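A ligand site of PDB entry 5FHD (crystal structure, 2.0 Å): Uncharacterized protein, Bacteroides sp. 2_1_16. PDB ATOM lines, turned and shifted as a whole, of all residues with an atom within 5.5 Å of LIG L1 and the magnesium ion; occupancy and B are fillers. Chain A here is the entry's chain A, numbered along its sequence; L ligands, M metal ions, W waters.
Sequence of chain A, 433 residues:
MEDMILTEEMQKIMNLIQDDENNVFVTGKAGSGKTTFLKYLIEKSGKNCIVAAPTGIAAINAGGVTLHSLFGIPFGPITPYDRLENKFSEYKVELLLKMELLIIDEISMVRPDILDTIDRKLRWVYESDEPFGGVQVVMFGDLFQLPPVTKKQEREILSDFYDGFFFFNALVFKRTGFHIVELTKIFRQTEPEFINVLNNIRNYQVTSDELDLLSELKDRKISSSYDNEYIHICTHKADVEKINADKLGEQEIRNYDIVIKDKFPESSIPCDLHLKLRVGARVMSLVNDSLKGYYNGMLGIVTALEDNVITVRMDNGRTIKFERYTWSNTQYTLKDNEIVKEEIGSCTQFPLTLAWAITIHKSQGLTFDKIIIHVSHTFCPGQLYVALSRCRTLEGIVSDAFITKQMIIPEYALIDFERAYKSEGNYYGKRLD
Water W4 lies within hydrogen-bond range of the side-chain carboxylate (OE2) of Glu 106 (2.7 Å) and the side-chain carboxylate (OD2) of Asp 105 (3.3 Å). Water W6 lies within hydrogen-bond range of the backbone carbonyl oxygen of Gly 365 (2.7 Å), an oxygen (O4) of LIG L1 (2.7 Å) and the side-chain amide oxygen of Asn 61 (3.2 Å). Water W2 lies within hydrogen-bond range of O4 of LIG L1 (2.6 Å) and OD1 of Asn 61 (3.2 Å). Water W5 lies within hydrogen-bond range of O of Gly 33 (2.9 Å), N2 of LIG L1 (2.9 Å) and N of Phe 37 (3.5 Å). Water W3 lies within hydrogen-bond range of O of Gly 365 (2.7 Å), OG1 of Thr 367 (2.8 Å) and O4 of LIG L1 (3.2 Å).
The magnesium ion is bound by a fluorine (F3) of LG2 L2. O3 of LIG L1 binds the magnesium ion (2.0 Å). The magnesium ion is bound by water W6. The magnesium ion is bound by OG1 of Thr 35 (2.1 Å). The magnesium ion is bound by water W4, 2.1 Å away. The magnesium ion is bound by water W7 (2.2 Å).
Residues that only touch LIG L1: Met 4, Phe 187, Thr 367, Met 10, Asp 3 and Lys 29. Hydrophobic or aromatic side chains that line LIG L1: Met 4, Ile 5, Met 10 and Phe 187. Of the 24 residues printed, 15 come within 4 Å of LIG L1. Along chain A the residues within 4 Å of LIG L1 span positions 3 to 392.
OG1 of Thr 35 lies close to OD2 of Asp 105, at 2.5 Å. NZ of Lys 34 sits at hydrogen-bond distance from O of Lys 29. The backbone carbonyl oxygen (O) of Gly 31 sits at hydrogen-bond distance from the backbone NH (N) of Arg 188 (3.1 Å). The backbone carbonyl oxygen (O) of Gly 31 lies within hydrogen-bond range of the backbone NH (N) of Phe 187 (2.8 Å). OG of Ser 32 lies within hydrogen-bond range of O of Lys 29 (2.6 Å). The guanidinium group (NE) of Arg 188 is in hydrogen-bond range of the side-chain hydroxyl (OG1) of Thr 367. OE2 of Glu 106 sits close to N of Gly 365 (3.2 Å).
Asp 105 touches the magnesium ion (OD2 to MG, 3.9 Å). Glu 106 touches the magnesium ion (OE2 to MG, 3.8 Å). Three residues have an atom within 4 Å of the magnesium ion: Thr 35, Asp 105 and Glu 106. The nearest printed residue that does not touch the magnesium ion is Gly 365 (4.4 Å).
An oxygen (O1) of LIG L1 is bound to an aluminium atom (AL1) of LG2 L2, at 2.0 Å.
N of Thr 35 lies within hydrogen-bond range of O5 of LIG L1, at 3.4 Å. The backbone NH (N) of Thr 36 sits at hydrogen-bond distance from an oxygen (O5) of LIG L1. An oxygen (O5) of LIG L1 lies within hydrogen-bond range of the side-chain hydroxyl (OG1) of Thr 36. An oxygen (O2) of LIG L1 lies within hydrogen-bond range of the backbone NH (N) of Lys 34 (2.8 Å). NZ of Lys 34 lies within salt-bridge range of O2 of LIG L1, at 2.7 Å. The backbone NH (N) of Ile 5 sits at hydrogen-bond distance from a nitrogen (N4) of LIG L1 (2.9 Å). A nitrogen (N3) of LIG L1 sits at hydrogen-bond distance from the backbone carbonyl oxygen (O) of Ile 5 (2.7 Å). An oxygen (O10) of LIG L1 is in hydrogen-bond range of the guanidinium group (NH1) of Arg 392 (2.9 Å). An oxygen (O1) of LIG L1 lies close to the backbone NH (N) of Gly 31 (2.9 Å). O2 of LIG L1 lies within hydrogen-bond range of N of Gly 33 (3.1 Å). O2 of LIG L1 sits at hydrogen-bond distance from N of Ser 32, 3.2 Å away. NH2 of Arg 188 is in salt-bridge range of O4 of LIG L1 (3.3 Å). The side-chain amino group (NZ) of Lys 34 sits at hydrogen-bond distance from a fluorine (F2) of LG2 L2 (2.6 Å). A fluorine (F4) of LG2 L2 lies within hydrogen-bond range of the backbone NH of Gly 31 (3.1 Å). F1 of LG2 L2 sits at hydrogen-bond distance from NH2 of Arg 188, at 2.7 Å. NH2 of Arg 390 sits at hydrogen-bond distance from F4 of LG2 L2 (2.8 Å). A fluorine (F2) of LG2 L2 is in hydrogen-bond range of the side-chain amide nitrogen of Gln 145 (2.9 Å).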
ATOM      1  N   ASP A   3      35.912  24.626   8.231  1.00  0.00           N
ATOM      2  CA  ASP A   3      35.367  23.345   7.791  1.00  0.00           C
ATOM      3  C   ASP A   3      33.971  23.534   7.190  1.00  0.00           C
ATOM      4  O   ASP A   3      33.343  22.564   6.746  1.00  0.00           O
ATOM      5  CB  ASP A   3      35.309  22.356   8.954  1.00  0.00           C
ATOM      6  CG  ASP A   3      34.593  22.924  10.145  1.00  0.00           C
ATOM      7  OD1 ASP A   3      34.469  24.170  10.205  1.00  0.00           O
ATOM      8  OD2 ASP A   3      34.161  22.146  11.029  1.00  0.00           O
ATOM      9  N   MET A   4      33.464  24.761   7.204  1.00  0.00           N
ATOM     10  CA  MET A   4      32.241  25.096   6.492  1.00  0.00           C
ATOM     11  C   MET A   4      32.517  25.084   5.000  1.00  0.00           C
ATOM     12  O   MET A   4      33.483  25.701   4.545  1.00  0.00           O
ATOM     13  CB  MET A   4      31.740  26.488   6.889  1.00  0.00           C
ATOM     14  CG  MET A   4      30.363  26.875   6.254  1.00  0.00           C
ATOM     15  SD  MET A   4      30.108  28.566   5.631  1.00  0.00           S
ATOM     16  CE  MET A   4      30.531  29.508   7.087  1.00  0.00           C
ATOM     17  N   ILE A   5      31.700  24.389   4.227  1.00  0.00           N
ATOM     18  CA  ILE A   5      31.844  24.361   2.785  1.00  0.00           C
ATOM     19  C   ILE A   5      30.986  25.462   2.180  1.00  0.00           C
ATOM     20  O   ILE A   5      29.777  25.514   2.421  1.00  0.00           O
ATOM     21  CB  ILE A   5      31.437  22.975   2.250  1.00  0.00           C
ATOM     22  CG1 ILE A   5      32.430  21.912   2.738  1.00  0.00           C
ATOM     23  CG2 ILE A   5      31.237  23.021   0.738  1.00  0.00           C
ATOM     24  CD1 ILE A   5      31.828  20.513   2.833  1.00  0.00           C
ATOM     25  N   LEU A   6      31.581  26.322   1.369  1.00  0.00           N
ATOM     26  CA  LEU A   6      30.798  27.291   0.605  1.00  0.00           C
ATOM     27  C   LEU A   6      30.465  26.704  -0.768  1.00  0.00           C
ATOM     28  O   LEU A   6      31.355  26.574  -1.619  1.00  0.00           O
ATOM     29  CB  LEU A   6      31.558  28.610   0.464  1.00  0.00           C
ATOM     30  CG  LEU A   6      30.787  29.737  -0.234  1.00  0.00           C
ATOM     31  CD1 LEU A   6      29.609  30.157   0.630  1.00  0.00           C
ATOM     32  CD2 LEU A   6      31.727  30.939  -0.525  1.00  0.00           C
ATOM     33  N   MET A  10      25.355  28.546  -2.721  1.00  0.00           N
ATOM     34  CA  MET A  10      25.459  29.619  -1.731  1.00  0.00           C
ATOM     35  C   MET A  10      26.088  30.860  -2.331  1.00  0.00           C
ATOM     36  O   MET A  10      25.705  31.997  -2.001  1.00  0.00           O
ATOM     37  CB  MET A  10      26.302  29.165  -0.530  1.00  0.00           C
ATOM     38  CG  MET A  10      25.618  28.101   0.316  1.00  0.00           C
ATOM     39  SD  MET A  10      26.834  27.266   1.360  1.00  0.00           S
ATOM     40  CE  MET A  10      25.868  25.768   1.836  1.00  0.00           C
ATOM     41  N   LYS A  29      15.823  21.655   2.380  1.00  0.00           N
ATOM     42  CA  LYS A  29      15.391  20.652   3.346  1.00  0.00           C
ATOM     43  C   LYS A  29      16.134  20.811   4.688  1.00  0.00           C
ATOM     44  O   LYS A  29      17.042  21.634   4.845  1.00  0.00           O
ATOM     45  CB  LYS A  29      15.595  19.266   2.752  1.00  0.00           C
ATOM     46  CG  LYS A  29      14.849  19.077   1.412  1.00  0.00           C
ATOM     47  CD  LYS A  29      15.139  17.694   0.867  1.00  0.00           C
ATOM     48  CE  LYS A  29      14.564  17.484  -0.552  1.00  0.00           C
ATOM     49  NZ  LYS A  29      15.670  17.421  -1.543  1.00  0.00           N
ATOM     50  N   ALA A  30      15.674  20.063   5.700  1.00  0.00           N
ATOM     51  CA  ALA A  30      16.332  20.083   7.022  1.00  0.00           C
ATOM     52  C   ALA A  30      17.822  19.834   6.872  1.00  0.00           C
ATOM     53  O   ALA A  30      18.248  18.916   6.149  1.00  0.00           O
ATOM     54  CB  ALA A  30      15.743  19.006   7.950  1.00  0.00           C
ATOM     55  N   GLY A  31      18.630  20.659   7.563  1.00  0.00           N
ATOM     56  CA  GLY A  31      20.072  20.382   7.644  1.00  0.00           C
ATOM     57  C   GLY A  31      20.805  20.599   6.332  1.00  0.00           C
ATOM     58  O   GLY A  31      21.894  20.043   6.136  1.00  0.00           O
ATOM     59  N   SER A  32      20.260  21.445   5.443  1.00  0.00           N
ATOM     60  CA  SER A  32      20.933  21.826   4.213  1.00  0.00           C
ATOM     61  C   SER A  32      21.821  23.028   4.401  1.00  0.00           C
ATOM     62  O   SER A  32      22.323  23.591   3.417  1.00  0.00           O
ATOM     63  CB  SER A  32      19.899  22.098   3.101  1.00  0.00           C
ATOM     64  OG  SER A  32      18.894  22.975   3.562  1.00  0.00           O
ATOM     65  N   GLY A  33      22.069  23.443   5.627  1.00  0.00           N
ATOM     66  CA  GLY A  33      22.974  24.567   5.829  1.00  0.00           C
ATOM     67  C   GLY A  33      22.335  25.930   5.773  1.00  0.00           C
ATOM     68  O   GLY A  33      23.053  26.922   5.598  1.00  0.00           O
ATOM     69  N   LYS A  34      21.017  26.040   5.927  1.00  0.00           N
ATOM     70  CA  LYS A  34      20.383  27.343   5.759  1.00  0.00           C
ATOM     71  C   LYS A  34      20.840  28.337   6.824  1.00  0.00           C
ATOM     72  O   LYS A  34      21.202  29.485   6.520  1.00  0.00           O
ATOM     73  CB  LYS A  34      18.840  27.210   5.786  1.00  0.00           C
ATOM     74  CG  LYS A  34      18.305  26.438   4.578  1.00  0.00           C
ATOM     75  CD  LYS A  34      16.747  26.363   4.555  1.00  0.00           C
ATOM     76  CE  LYS A  34      16.222  25.612   5.785  1.00  0.00           C
ATOM     77  NZ  LYS A  34      16.750  24.271   6.087  1.00  0.00           N
ATOM     78  N   THR A  35      20.783  27.927   8.084  1.00  0.00           N
ATOM     79  CA  THR A  35      21.138  28.880   9.154  1.00  0.00           C
ATOM     80  C   THR A  35      22.636  29.114   9.176  1.00  0.00           C
ATOM     81  O   THR A  35      23.087  30.234   9.471  1.00  0.00           O
ATOM     82  CB  THR A  35      20.644  28.327  10.512  1.00  0.00           C
ATOM     83  OG1 THR A  35      19.217  28.230  10.510  1.00  0.00           O
ATOM     84  CG2 THR A  35      21.062  29.249  11.680  1.00  0.00           C
ATOM     85  N   THR A  36      23.421  28.067   8.876  1.00  0.00           N
ATOM     86  CA  THR A  36      24.871  28.243   8.707  1.00  0.00           C
ATOM     87  C   THR A  36      25.169  29.272   7.627  1.00  0.00           C
ATOM     88  O   THR A  36      26.044  30.141   7.791  1.00  0.00           O
ATOM     89  CB  THR A  36      25.526  26.898   8.391  1.00  0.00           C
ATOM     90  OG1 THR A  36      25.213  25.999   9.477  1.00  0.00           O
ATOM     91  CG2 THR A  36      27.109  27.036   8.305  1.00  0.00           C
ATOM     92  N   PHE A  37      24.450  29.210   6.506  1.00  0.00           N
ATOM     93  CA  PHE A  37      24.702  30.136   5.415  1.00  0.00           C
ATOM     94  C   PHE A  37      24.205  31.541   5.755  1.00  0.00           C
ATOM     95  O   PHE A  37      24.844  32.549   5.393  1.00  0.00           O
ATOM     96  CB  PHE A  37      24.034  29.586   4.147  1.00  0.00           C
ATOM     97  CG  PHE A  37      24.032  30.547   2.995  1.00  0.00           C
ATOM     98  CD1 PHE A  37      25.238  31.026   2.461  1.00  0.00           C
ATOM     99  CD2 PHE A  37      22.840  30.952   2.431  1.00  0.00           C
ATOM    100  CE1 PHE A  37      25.242  31.951   1.391  1.00  0.00           C
ATOM    101  CE2 PHE A  37      22.817  31.859   1.348  1.00  0.00           C
ATOM    102  CZ  PHE A  37      24.029  32.364   0.846  1.00  0.00           C
ATOM    103  N   ASN A  61      19.724  30.431  17.967  1.00  0.00           N
ATOM    104  CA  ASN A  61      20.537  29.637  17.029  1.00  0.00           C
ATOM    105  C   ASN A  61      21.029  30.430  15.823  1.00  0.00           C
ATOM    106  O   ASN A  61      22.128  30.156  15.296  1.00  0.00           O
ATOM    107  CB  ASN A  61      19.704  28.443  16.542  1.00  0.00           C
ATOM    108  CG  ASN A  61      20.471  27.498  15.673  1.00  0.00           C
ATOM    109  OD1 ASN A  61      20.138  27.279  14.493  1.00  0.00           O
ATOM    110  ND2 ASN A  61      21.482  26.924  16.240  1.00  0.00           N
ATOM    111  N   ASP A 105      14.827  33.873  10.246  1.00  0.00           N
ATOM    112  CA  ASP A 105      15.044  32.420  10.138  1.00  0.00           C
ATOM    113  C   ASP A 105      13.796  31.652  10.567  1.00  0.00           C
ATOM    114  O   ASP A 105      12.890  32.200  11.216  1.00  0.00           O
ATOM    115  CB  ASP A 105      16.255  31.973  10.999  1.00  0.00           C
ATOM    116  CG  ASP A 105      16.921  30.682  10.509  1.00  0.00           C
ATOM    117  OD1 ASP A 105      16.419  30.055   9.546  1.00  0.00           O
ATOM    118  OD2 ASP A 105      17.958  30.266  11.084  1.00  0.00           O
ATOM    119  N   GLU A 106      13.738  30.365  10.194  1.00  0.00           N
ATOM    120  CA  GLU A 106      12.567  29.509  10.475  1.00  0.00           C
ATOM    121  C   GLU A 106      11.248  30.204  10.058  1.00  0.00           C
ATOM    122  O   GLU A 106      10.244  30.250  10.797  1.00  0.00           O
ATOM    123  CB  GLU A 106      12.541  29.063  11.939  1.00  0.00           C
ATOM    124  CG  GLU A 106      13.717  28.057  12.310  1.00  0.00           C
ATOM    125  CD  GLU A 106      13.748  26.713  11.536  1.00  0.00           C
ATOM    126  OE1 GLU A 106      12.892  26.460  10.653  1.00  0.00           O
ATOM    127  OE2 GLU A 106      14.653  25.875  11.818  1.00  0.00           O
ATOM    128  N   GLN A 145       8.482  21.916   7.292  1.00  0.00           N
ATOM    129  CA  GLN A 145       8.676  21.656   8.725  1.00  0.00           C
ATOM    130  C   GLN A 145       7.469  22.237   9.442  1.00  0.00           C
ATOM    131  O   GLN A 145       6.382  22.217   8.860  1.00  0.00           O
ATOM    132  CB  GLN A 145      10.011  22.240   9.195  1.00  0.00           C
ATOM    133  CG  GLN A 145      11.174  21.424   8.519  1.00  0.00           C
ATOM    134  CD  GLN A 145      12.569  21.948   8.869  1.00  0.00           C
ATOM    135  OE1 GLN A 145      12.792  22.376  10.004  1.00  0.00           O
ATOM    136  NE2 GLN A 145      13.500  21.929   7.903  1.00  0.00           N
ATOM    137  N   PHE A 187      23.734  18.530   4.685  1.00  0.00           N
ATOM    138  CA  PHE A 187      24.958  18.397   5.475  1.00  0.00           C
ATOM    139  C   PHE A 187      24.769  17.658   6.798  1.00  0.00           C
ATOM    140  O   PHE A 187      25.685  16.952   7.247  1.00  0.00           O
ATOM    141  CB  PHE A 187      25.523  19.776   5.781  1.00  0.00           C
ATOM    142  CG  PHE A 187      26.046  20.485   4.581  1.00  0.00           C
ATOM    143  CD1 PHE A 187      27.244  20.082   3.980  1.00  0.00           C
ATOM    144  CD2 PHE A 187      25.363  21.578   4.062  1.00  0.00           C
ATOM    145  CE1 PHE A 187      27.730  20.753   2.847  1.00  0.00           C
ATOM    146  CE2 PHE A 187      25.851  22.239   2.939  1.00  0.00           C
ATOM    147  CZ  PHE A 187      27.035  21.818   2.342  1.00  0.00           C
ATOM    148  N   ARG A 188      23.638  17.869   7.464  1.00  0.00           N
ATOM    149  CA  ARG A 188      23.461  17.339   8.813  1.00  0.00           C
ATOM    150  C   ARG A 188      23.533  15.812   8.829  1.00  0.00           C
ATOM    151  O   ARG A 188      24.246  15.226   9.646  1.00  0.00           O
ATOM    152  CB  ARG A 188      22.141  17.829   9.412  1.00  0.00           C
ATOM    153  CG  ARG A 188      21.894  17.312  10.859  1.00  0.00           C
ATOM    154  CD  ARG A 188      20.591  17.827  11.432  1.00  0.00           C
ATOM    155  NE  ARG A 188      20.647  19.288  11.646  1.00  0.00           N
ATOM    156  CZ  ARG A 188      19.648  20.130  11.351  1.00  0.00           C
ATOM    157  NH1 ARG A 188      18.504  19.677  10.832  1.00  0.00           N
ATOM    158  NH2 ARG A 188      19.807  21.426  11.576  1.00  0.00           N
ATOM    159  N   GLY A 365      15.356  23.762  14.175  1.00  0.00           N
ATOM    160  CA  GLY A 365      16.566  24.555  14.024  1.00  0.00           C
ATOM    161  C   GLY A 365      17.813  23.925  14.645  1.00  0.00           C
ATOM    162  O   GLY A 365      18.924  24.258  14.200  1.00  0.00           O
ATOM    163  N   THR A 367      20.491  20.736  16.050  1.00  0.00           N
ATOM    164  CA  THR A 367      21.104  19.490  15.638  1.00  0.00           C
ATOM    165  C   THR A 367      21.534  18.733  16.893  1.00  0.00           C
ATOM    166  O   THR A 367      21.994  19.355  17.857  1.00  0.00           O
ATOM    167  CB  THR A 367      22.363  19.743  14.764  1.00  0.00           C
ATOM    168  OG1 THR A 367      22.038  20.536  13.615  1.00  0.00           O
ATOM    169  CG2 THR A 367      22.930  18.446  14.301  1.00  0.00           C
ATOM    170  N   ARG A 390      16.337  16.081  13.306  1.00  0.00           N
ATOM    171  CA  ARG A 390      17.261  16.749  14.234  1.00  0.00           C
ATOM    172  C   ARG A 390      18.567  15.989  14.382  1.00  0.00           C
ATOM    173  O   ARG A 390      19.579  16.575  14.789  1.00  0.00           O
ATOM    174  CB  ARG A 390      16.648  16.889  15.646  1.00  0.00           C
ATOM    175  CG  ARG A 390      15.323  17.627  15.771  1.00  0.00           C
ATOM    176  CD  ARG A 390      15.441  19.031  15.125  1.00  0.00           C
ATOM    177  NE  ARG A 390      15.159  18.988  13.686  1.00  0.00           N
ATOM    178  CZ  ARG A 390      15.544  19.931  12.825  1.00  0.00           C
ATOM    179  NH1 ARG A 390      16.330  20.946  13.220  1.00  0.00           N
ATOM    180  NH2 ARG A 390      15.157  19.854  11.560  1.00  0.00           N
ATOM    181  N   ARG A 392      21.954  13.602  13.636  1.00  0.00           N
ATOM    182  CA  ARG A 392      22.936  13.424  12.566  1.00  0.00           C
ATOM    183  C   ARG A 392      22.929  12.020  12.002  1.00  0.00           C
ATOM    184  O   ARG A 392      23.274  11.848  10.836  1.00  0.00           O
ATOM    185  CB  ARG A 392      24.338  13.789  13.058  1.00  0.00           C
ATOM    186  CG  ARG A 392      24.476  15.258  13.492  1.00  0.00           C
ATOM    187  CD  ARG A 392      25.963  15.581  13.742  1.00  0.00           C
ATOM    188  NE  ARG A 392      26.130  16.937  14.241  1.00  0.00           N
ATOM    189  CZ  ARG A 392      26.277  17.981  13.426  1.00  0.00           C
ATOM    190  NH1 ARG A 392      26.307  17.787  12.106  1.00  0.00           N
ATOM    191  NH2 ARG A 392      26.418  19.183  13.941  1.00  0.00           N
HETATM  192  P1  LIG L   1      19.460  24.121   8.435  1.00  0.00           P
HETATM  193  O1  LIG L   1      18.540  23.150   9.098  1.00  0.00           O
HETATM  194  O2  LIG L   1      19.308  24.058   6.941  1.00  0.00           O
HETATM  195  O3  LIG L   1      19.344  25.429   9.033  1.00  0.00           O
HETATM  196  P2  LIG L   1      22.088  24.083   9.682  1.00  0.00           P
HETATM  197  O4  LIG L   1      21.591  24.140  11.090  1.00  0.00           O
HETATM  198  O5  LIG L   1      22.694  25.332   9.102  1.00  0.00           O
HETATM  199  O6  LIG L   1      20.923  23.466   8.764  1.00  0.00           O
HETATM  200  O7  LIG L   1      23.159  22.869   9.530  1.00  0.00           O
HETATM  201  C1  LIG L   1      23.103  21.724  10.404  1.00  0.00           C
HETATM  202  C2  LIG L   1      24.475  21.061  10.468  1.00  0.00           C
HETATM  203  O8  LIG L   1      24.932  20.810   9.147  1.00  0.00           O
HETATM  204  C3  LIG L   1      25.523  22.002  11.042  1.00  0.00           C
HETATM  205  O9  LIG L   1      25.467  21.864  12.436  1.00  0.00           O
HETATM  206  C4  LIG L   1      26.819  21.529  10.393  1.00  0.00           C
HETATM  207  O10 LIG L   1      27.265  20.286  10.979  1.00  0.00           O
HETATM  208  C5  LIG L   1      26.333  21.110   9.031  1.00  0.00           C
HETATM  209  N1  LIG L   1      26.493  22.178   8.014  1.00  0.00           N
HETATM  210  C6  LIG L   1      25.620  23.155   7.674  1.00  0.00           C
HETATM  211  N2  LIG L   1      26.129  23.918   6.679  1.00  0.00           N
HETATM  212  C7  LIG L   1      27.344  23.420   6.374  1.00  0.00           C
HETATM  213  C8  LIG L   1      28.413  23.765   5.426  1.00  0.00           C
HETATM  214  N3  LIG L   1      28.281  24.805   4.575  1.00  0.00           N
HETATM  215  N4  LIG L   1      29.516  22.996   5.417  1.00  0.00           N
HETATM  216  C9  LIG L   1      29.649  21.942   6.255  1.00  0.00           C
HETATM  217  N5  LIG L   1      28.718  21.563   7.164  1.00  0.00           N
HETATM  218  C10 LIG L   1      27.573  22.280   7.256  1.00  0.00           C
HETATM  219 AL1  LG2 L   2      16.761  23.227   9.995  1.00  0.00          AL
HETATM  220  F1  LG2 L   2      17.592  22.895  11.550  1.00  0.00           F
HETATM  221  F2  LG2 L   2      15.936  23.488   8.413  1.00  0.00           F
HETATM  222  F3  LG2 L   2      16.928  24.969  10.241  1.00  0.00           F
HETATM  223  F4  LG2 L   2      16.584  21.460   9.804  1.00  0.00           F
HETATM  224 MG    MG M   1      18.197  26.392  10.420  1.00  0.00          MG
HETATM  225  O   HOH W   1      29.568  19.141   8.071  1.00  0.00           O
HETATM  226  O   HOH W   2      22.427  25.689  12.991  1.00  0.00           O
HETATM  227  O   HOH W   3      21.408  23.225  14.120  1.00  0.00           O
HETATM  228  O   HOH W   4      17.001  27.187  11.968  1.00  0.00           O
HETATM  229  O   HOH W   5      25.787  26.337   5.029  1.00  0.00           O
HETATM  230  O   HOH W   6      19.419  25.537  11.898  1.00  0.00           O
HETATM  231  O   HOH W   7      16.933  27.488   8.957  1.00  0.00           O
HETATM  232  O   HOH W   8      29.871  20.781  12.062  1.00  0.00           O
